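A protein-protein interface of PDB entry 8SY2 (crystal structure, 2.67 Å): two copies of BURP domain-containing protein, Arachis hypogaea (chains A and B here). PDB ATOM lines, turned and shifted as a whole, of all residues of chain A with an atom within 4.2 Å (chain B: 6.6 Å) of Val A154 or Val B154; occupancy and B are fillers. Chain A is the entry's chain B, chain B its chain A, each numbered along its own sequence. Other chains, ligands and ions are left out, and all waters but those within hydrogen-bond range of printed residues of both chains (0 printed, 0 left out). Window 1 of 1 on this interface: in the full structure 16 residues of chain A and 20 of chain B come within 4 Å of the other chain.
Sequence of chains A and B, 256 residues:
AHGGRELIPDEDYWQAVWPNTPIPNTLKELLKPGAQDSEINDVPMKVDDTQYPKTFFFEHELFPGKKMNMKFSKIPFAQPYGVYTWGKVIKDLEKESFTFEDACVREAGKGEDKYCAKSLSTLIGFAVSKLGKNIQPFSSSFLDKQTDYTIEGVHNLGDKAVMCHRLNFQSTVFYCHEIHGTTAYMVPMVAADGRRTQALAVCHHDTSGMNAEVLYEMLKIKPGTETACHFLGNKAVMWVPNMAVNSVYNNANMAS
Printed residues of chain B that touch a printed residue of chain A: Leu B62, Phe B63, Pro B64, Glu B152, Gly B153, Val B154, His B155 and Tyr B185.
Among the printed residues, 14 pairs touch across the chains.
Among the printed residues, no Asp or Glu carboxylate lies within 4 Å of a Lys or Arg side-chain nitrogen of the other chain.
The backbone NH (N) of His A155 lies within hydrogen-bond range of the backbone carbonyl oxygen (O) of Met A186, 2.9 Å away.
N of Glu B152 sits at hydrogen-bond distance from O of Pro B188 (2.8 Å).
The backbone NH (N) of His B155 sits at hydrogen-bond distance from the backbone carbonyl oxygen (O) of Met B186 (2.9 Å).
Of the printed residues of chain B, Pro A64 touches Leu B62 (3.4 Å) and Tyr B185 (3.3 Å).
Of chain B, only Pro B64 (3.95 Å), Gly B153 (3.4 Å) and Val B154 (2.7 Å) come within 4 Å of Val A154.
Of the printed residues of chain A, Tyr B185 touches Pro A64.
The nearest printed residue of chain A that does not touch Val B154 is Pro A64 (4.03 Å).
The nearest printed residue of chain B that does not touch Asn A156 is Gly B153 (4.7 Å).
Leu A62 touches its own counterpart, Leu B62.
Pro A64 touches Tyr B185, and with the chains exchanged Tyr A185 touches Pro B64.
Val A154 touches Pro B64, but with the chains exchanged Pro A64 does not touch Val B154 (4.03 Å).
His A155 touches Val B154, but with the chains exchanged Val A154 does not touch His B155 (4.3 Å).
Positions printed for both chains: 62, 64, 153, 154, 155, 156, 185 and 186.
The backbone carbonyl oxygen (O) of Glu B152 is in hydrogen-bond range of the side-chain amide nitrogen (ND2) of Asn A156 (2.9 Å).
N of Val B154 sits at hydrogen-bond distance from O of Val A154.
A ring nitrogen (ND1) of His B155 sits at hydrogen-bond distance from a ring nitrogen (ND1) of His A155 (2.9 Å).
Among the printed residues, merely in contact across the chains: Tyr A185 with Pro B64 (3.2 Å), Pro A64 with Tyr B185 (3.3 Å), Leu A62 with Phe B63 (3.3 Å), Leu A62 with Pro B64 (3.4 Å), Pro A64 with Leu B62 (3.4 Å), Val A154 with Gly B153 (3.4 Å), Gly A153 with Val B154 (3.5 Å), Leu A62 with Leu B62 (3.8 Å), Tyr A185 with Glu B152 (3.9 Å), Val A154 with Pro B64 (3.95 Å) and His A155 with Val B154 (3.99 Å).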
ATOM      1  N   LEU A  62     -17.840  22.907  18.005  1.00  0.00           N
ATOM      2  CA  LEU A  62     -17.811  21.560  18.540  1.00  0.00           C
ATOM      3  C   LEU A  62     -18.393  21.560  19.942  1.00  0.00           C
ATOM      4  O   LEU A  62     -17.660  21.739  20.899  1.00  0.00           O
ATOM      5  CB  LEU A  62     -16.360  21.098  18.567  1.00  0.00           C
ATOM      6  CG  LEU A  62     -15.756  20.923  17.184  1.00  0.00           C
ATOM      7  CD1 LEU A  62     -14.274  20.633  17.253  1.00  0.00           C
ATOM      8  CD2 LEU A  62     -16.470  19.814  16.447  1.00  0.00           C
ATOM      9  N   PRO A  64     -21.849  19.859  22.617  1.00  0.00           N
ATOM     10  CA  PRO A  64     -22.921  18.889  22.718  1.00  0.00           C
ATOM     11  C   PRO A  64     -24.212  19.505  22.223  1.00  0.00           C
ATOM     12  O   PRO A  64     -24.665  20.515  22.739  1.00  0.00           O
ATOM     13  CB  PRO A  64     -23.022  18.581  24.212  1.00  0.00           C
ATOM     14  CG  PRO A  64     -21.693  18.997  24.753  1.00  0.00           C
ATOM     15  CD  PRO A  64     -21.280  20.186  23.920  1.00  0.00           C
ATOM     16  N   GLY A 153     -20.263  14.625  22.083  1.00  0.00           N
ATOM     17  CA  GLY A 153     -19.170  15.113  22.907  1.00  0.00           C
ATOM     18  C   GLY A 153     -17.938  15.394  22.063  1.00  0.00           C
ATOM     19  O   GLY A 153     -17.974  15.202  20.861  1.00  0.00           O
ATOM     20  N   VAL A 154     -16.832  15.758  22.707  1.00  0.00           N
ATOM     21  CA  VAL A 154     -15.629  16.134  21.987  1.00  0.00           C
ATOM     22  C   VAL A 154     -14.422  15.775  22.833  1.00  0.00           C
ATOM     23  O   VAL A 154     -14.247  16.347  23.903  1.00  0.00           O
ATOM     24  CB  VAL A 154     -15.584  17.651  21.739  1.00  0.00           C
ATOM     25  CG1 VAL A 154     -14.443  18.024  20.821  1.00  0.00           C
ATOM     26  CG2 VAL A 154     -16.895  18.161  21.204  1.00  0.00           C
ATOM     27  N   HIS A 155     -13.545  14.939  22.300  1.00  0.00           N
ATOM     28  CA  HIS A 155     -12.438  14.443  23.087  1.00  0.00           C
ATOM     29  C   HIS A 155     -11.153  14.938  22.461  1.00  0.00           C
ATOM     30  O   HIS A 155     -10.902  14.702  21.287  1.00  0.00           O
ATOM     31  CB  HIS A 155     -12.413  12.913  23.131  1.00  0.00           C
ATOM     32  CG  HIS A 155     -13.656  12.276  23.631  1.00  0.00           C
ATOM     33  ND1 HIS A 155     -14.410  12.761  24.673  1.00  0.00           N
ATOM     34  CD2 HIS A 155     -14.266  11.191  23.224  1.00  0.00           C
ATOM     35  CE1 HIS A 155     -15.452  11.968  24.869  1.00  0.00           C
ATOM     36  NE2 HIS A 155     -15.392  11.023  23.988  1.00  0.00           N
ATOM     37  N   ASN A 156     -10.324  15.569  23.285  1.00  0.00           N
ATOM     38  CA  ASN A 156      -9.083  16.140  22.822  1.00  0.00           C
ATOM     39  C   ASN A 156      -8.020  15.058  22.660  1.00  0.00           C
ATOM     40  O   ASN A 156      -7.732  14.359  23.614  1.00  0.00           O
ATOM     41  CB  ASN A 156      -8.671  17.146  23.867  1.00  0.00           C
ATOM     42  CG  ASN A 156      -7.571  18.050  23.385  1.00  0.00           C
ATOM     43  OD1 ASN A 156      -6.539  17.587  22.912  1.00  0.00           O
ATOM     44  ND2 ASN A 156      -7.800  19.344  23.503  1.00  0.00           N
ATOM     45  N   TYR A 185      -9.213  15.809  17.288  1.00  0.00           N
ATOM     46  CA  TYR A 185     -10.302  15.552  18.200  1.00  0.00           C
ATOM     47  C   TYR A 185     -11.066  14.319  17.763  1.00  0.00           C
ATOM     48  O   TYR A 185     -11.153  14.054  16.578  1.00  0.00           O
ATOM     49  CB  TYR A 185     -11.266  16.729  18.175  1.00  0.00           C
ATOM     50  CG  TYR A 185     -10.767  17.985  18.832  1.00  0.00           C
ATOM     51  CD1 TYR A 185     -10.897  18.191  20.196  1.00  0.00           C
ATOM     52  CD2 TYR A 185     -10.207  18.989  18.077  1.00  0.00           C
ATOM     53  CE1 TYR A 185     -10.484  19.369  20.792  1.00  0.00           C
ATOM     54  CE2 TYR A 185      -9.783  20.174  18.656  1.00  0.00           C
ATOM     55  CZ  TYR A 185      -9.923  20.364  20.014  1.00  0.00           C
ATOM     56  OH  TYR A 185      -9.491  21.545  20.538  1.00  0.00           O
ATOM     57  N   MET A 186     -11.665  13.622  18.722  1.00  0.00           N
ATOM     58  CA  MET A 186     -12.565  12.536  18.404  1.00  0.00           C
ATOM     59  C   MET A 186     -13.952  13.015  18.787  1.00  0.00           C
ATOM     60  O   MET A 186     -14.109  13.528  19.886  1.00  0.00           O
ATOM     61  CB  MET A 186     -12.175  11.297  19.205  1.00  0.00           C
ATOM     62  CG  MET A 186     -13.180  10.164  19.176  1.00  0.00           C
ATOM     63  SD  MET A 186     -13.414   9.534  17.518  1.00  0.00           S
ATOM     64  CE  MET A 186     -12.040   8.405  17.353  1.00  0.00           C
ATOM     65  N   LEU B  62     -20.034  24.674  26.259  1.00  0.00           N
ATOM     66  CA  LEU B  62     -19.038  23.642  26.489  1.00  0.00           C
ATOM     67  C   LEU B  62     -18.334  23.319  25.183  1.00  0.00           C
ATOM     68  O   LEU B  62     -18.797  22.470  24.434  1.00  0.00           O
ATOM     69  CB  LEU B  62     -19.759  22.409  27.016  1.00  0.00           C
ATOM     70  CG  LEU B  62     -20.337  22.580  28.411  1.00  0.00           C
ATOM     71  CD1 LEU B  62     -21.227  21.415  28.781  1.00  0.00           C
ATOM     72  CD2 LEU B  62     -19.213  22.703  29.410  1.00  0.00           C
ATOM     73  N   PHE B  63     -17.223  23.995  24.900  1.00  0.00           N
ATOM     74  CA  PHE B  63     -16.497  23.691  23.684  1.00  0.00           C
ATOM     75  C   PHE B  63     -15.008  23.932  23.872  1.00  0.00           C
ATOM     76  O   PHE B  63     -14.581  24.659  24.762  1.00  0.00           O
ATOM     77  CB  PHE B  63     -17.037  24.536  22.538  1.00  0.00           C
ATOM     78  CG  PHE B  63     -16.899  26.014  22.745  1.00  0.00           C
ATOM     79  CD1 PHE B  63     -15.749  26.674  22.338  1.00  0.00           C
ATOM     80  CD2 PHE B  63     -17.914  26.739  23.350  1.00  0.00           C
ATOM     81  CE1 PHE B  63     -15.618  28.042  22.516  1.00  0.00           C
ATOM     82  CE2 PHE B  63     -17.779  28.108  23.532  1.00  0.00           C
ATOM     83  CZ  PHE B  63     -16.633  28.755  23.119  1.00  0.00           C
ATOM     84  N   PRO B  64     -14.157  23.331  23.027  1.00  0.00           N
ATOM     85  CA  PRO B  64     -12.723  23.462  23.197  1.00  0.00           C
ATOM     86  C   PRO B  64     -12.320  24.909  23.011  1.00  0.00           C
ATOM     87  O   PRO B  64     -12.570  25.497  21.966  1.00  0.00           O
ATOM     88  CB  PRO B  64     -12.118  22.603  22.084  1.00  0.00           C
ATOM     89  CG  PRO B  64     -13.240  21.693  21.673  1.00  0.00           C
ATOM     90  CD  PRO B  64     -14.508  22.498  21.877  1.00  0.00           C
ATOM     91  N   ILE B 151     -11.377  25.257  28.479  1.00  0.00           N
ATOM     92  CA  ILE B 151     -11.904  23.921  28.318  1.00  0.00           C
ATOM     93  C   ILE B 151     -11.101  23.181  27.256  1.00  0.00           C
ATOM     94  O   ILE B 151     -10.852  23.705  26.187  1.00  0.00           O
ATOM     95  CB  ILE B 151     -13.389  24.026  27.968  1.00  0.00           C
ATOM     96  CG1 ILE B 151     -14.165  24.425  29.219  1.00  0.00           C
ATOM     97  CG2 ILE B 151     -13.877  22.735  27.352  1.00  0.00           C
ATOM     98  CD1 ILE B 151     -15.649  24.389  29.053  1.00  0.00           C
ATOM     99  N   GLU B 152     -10.696  21.954  27.558  1.00  0.00           N
ATOM    100  CA  GLU B 152      -9.889  21.175  26.639  1.00  0.00           C
ATOM    101  C   GLU B 152     -10.770  20.251  25.815  1.00  0.00           C
ATOM    102  O   GLU B 152     -10.430  19.912  24.692  1.00  0.00           O
ATOM    103  CB  GLU B 152      -8.911  20.271  27.381  1.00  0.00           C
ATOM    104  CG  GLU B 152      -7.882  21.016  28.206  1.00  0.00           C
ATOM    105  CD  GLU B 152      -6.723  20.162  28.710  1.00  0.00           C
ATOM    106  OE1 GLU B 152      -6.972  19.048  29.253  1.00  0.00           O
ATOM    107  OE2 GLU B 152      -5.559  20.609  28.568  1.00  0.00           O
ATOM    108  N   GLY B 153     -11.865  19.788  26.413  1.00  0.00           N
ATOM    109  CA  GLY B 153     -12.725  18.810  25.779  1.00  0.00           C
ATOM    110  C   GLY B 153     -13.941  18.566  26.656  1.00  0.00           C
ATOM    111  O   GLY B 153     -14.022  19.100  27.754  1.00  0.00           O
ATOM    112  N   VAL B 154     -14.876  17.750  26.170  1.00  0.00           N
ATOM    113  CA  VAL B 154     -16.133  17.545  26.865  1.00  0.00           C
ATOM    114  C   VAL B 154     -16.595  16.126  26.618  1.00  0.00           C
ATOM    115  O   VAL B 154     -16.899  15.770  25.478  1.00  0.00           O
ATOM    116  CB  VAL B 154     -17.206  18.497  26.325  1.00  0.00           C
ATOM    117  CG1 VAL B 154     -18.487  18.388  27.113  1.00  0.00           C
ATOM    118  CG2 VAL B 154     -16.710  19.918  26.302  1.00  0.00           C
ATOM    119  N   HIS B 155     -16.734  15.359  27.691  1.00  0.00           N
ATOM    120  CA  HIS B 155     -16.981  13.937  27.555  1.00  0.00           C
ATOM    121  C   HIS B 155     -18.361  13.657  28.110  1.00  0.00           C
ATOM    122  O   HIS B 155     -18.635  13.960  29.261  1.00  0.00           O
ATOM    123  CB  HIS B 155     -15.941  13.119  28.319  1.00  0.00           C
ATOM    124  CG  HIS B 155     -14.548  13.325  27.848  1.00  0.00           C
ATOM    125  ND1 HIS B 155     -13.743  12.293  27.443  1.00  0.00           N
ATOM    126  CD2 HIS B 155     -13.830  14.408  27.678  1.00  0.00           C
ATOM    127  CE1 HIS B 155     -12.574  12.774  27.056  1.00  0.00           C
ATOM    128  NE2 HIS B 155     -12.614  14.057  27.190  1.00  0.00           N
ATOM    129  N   ASN B 156     -19.192  13.030  27.290  1.00  0.00           N
ATOM    130  CA  ASN B 156     -20.557  12.753  27.650  1.00  0.00           C
ATOM    131  C   ASN B 156     -20.625  11.517  28.537  1.00  0.00           C
ATOM    132  O   ASN B 156     -20.178  10.472  28.121  1.00  0.00           O
ATOM    133  CB  ASN B 156     -21.315  12.490  26.369  1.00  0.00           C
ATOM    134  CG  ASN B 156     -22.805  12.586  26.574  1.00  0.00           C
ATOM    135  OD1 ASN B 156     -23.352  12.029  27.519  1.00  0.00           O
ATOM    136  ND2 ASN B 156     -23.472  13.291  25.684  1.00  0.00           N
ATOM    137  N   TYR B 185     -21.457  15.483  32.304  1.00  0.00           N
ATOM    138  CA  TYR B 185     -20.275  15.555  31.473  1.00  0.00           C
ATOM    139  C   TYR B 185     -19.034  15.597  32.336  1.00  0.00           C
ATOM    140  O   TYR B 185     -19.070  16.109  33.438  1.00  0.00           O
ATOM    141  CB  TYR B 185     -20.289  16.816  30.626  1.00  0.00           C
ATOM    142  CG  TYR B 185     -21.413  16.905  29.630  1.00  0.00           C
ATOM    143  CD1 TYR B 185     -22.642  17.429  29.974  1.00  0.00           C
ATOM    144  CD2 TYR B 185     -21.230  16.478  28.329  1.00  0.00           C
ATOM    145  CE1 TYR B 185     -23.663  17.519  29.044  1.00  0.00           C
ATOM    146  CE2 TYR B 185     -22.230  16.584  27.381  1.00  0.00           C
ATOM    147  CZ  TYR B 185     -23.456  17.099  27.745  1.00  0.00           C
ATOM    148  OH  TYR B 185     -24.463  17.173  26.827  1.00  0.00           O
ATOM    149  N   MET B 186     -17.926  15.132  31.780  1.00  0.00           N
ATOM    150  CA  MET B 186     -16.627  15.337  32.384  1.00  0.00           C
ATOM    151  C   MET B 186     -15.910  16.348  31.503  1.00  0.00           C
ATOM    152  O   MET B 186     -15.884  16.171  30.288  1.00  0.00           O
ATOM    153  CB  MET B 186     -15.866  14.015  32.402  1.00  0.00           C
ATOM    154  CG  MET B 186     -14.401  14.103  32.782  1.00  0.00           C
ATOM    155  SD  MET B 186     -14.169  14.477  34.535  1.00  0.00           S
ATOM    156  CE  MET B 186     -14.686  12.953  35.301  1.00  0.00           C
ATOM    157  N   VAL B 187     -15.374  17.407  32.116  1.00  0.00           N
ATOM    158  CA  VAL B 187     -14.886  18.545  31.364  1.00  0.00           C
ATOM    159  C   VAL B 187     -13.447  18.800  31.751  1.00  0.00           C
ATOM    160  O   VAL B 187     -13.154  19.374  32.789  1.00  0.00           O
ATOM    161  CB  VAL B 187     -15.721  19.804  31.614  1.00  0.00           C
ATOM    162  CG1 VAL B 187     -15.259  20.917  30.695  1.00  0.00           C
ATOM    163  CG2 VAL B 187     -17.198  19.536  31.442  1.00  0.00           C
ATOM    164  N   PRO B 188     -12.498  18.270  30.985  1.00  0.00           N
ATOM    165  CA  PRO B 188     -11.097  18.569  31.235  1.00  0.00           C
ATOM    166  C   PRO B 188     -10.789  20.023  30.907  1.00  0.00           C
ATOM    167  O   PRO B 188     -11.303  20.586  29.953  1.00  0.00           O
ATOM    168  CB  PRO B 188     -10.367  17.558  30.339  1.00  0.00           C
ATOM    169  CG  PRO B 188     -11.370  17.196  29.276  1.00  0.00           C
ATOM    170  CD  PRO B 188     -12.696  17.210  29.990  1.00  0.00           C
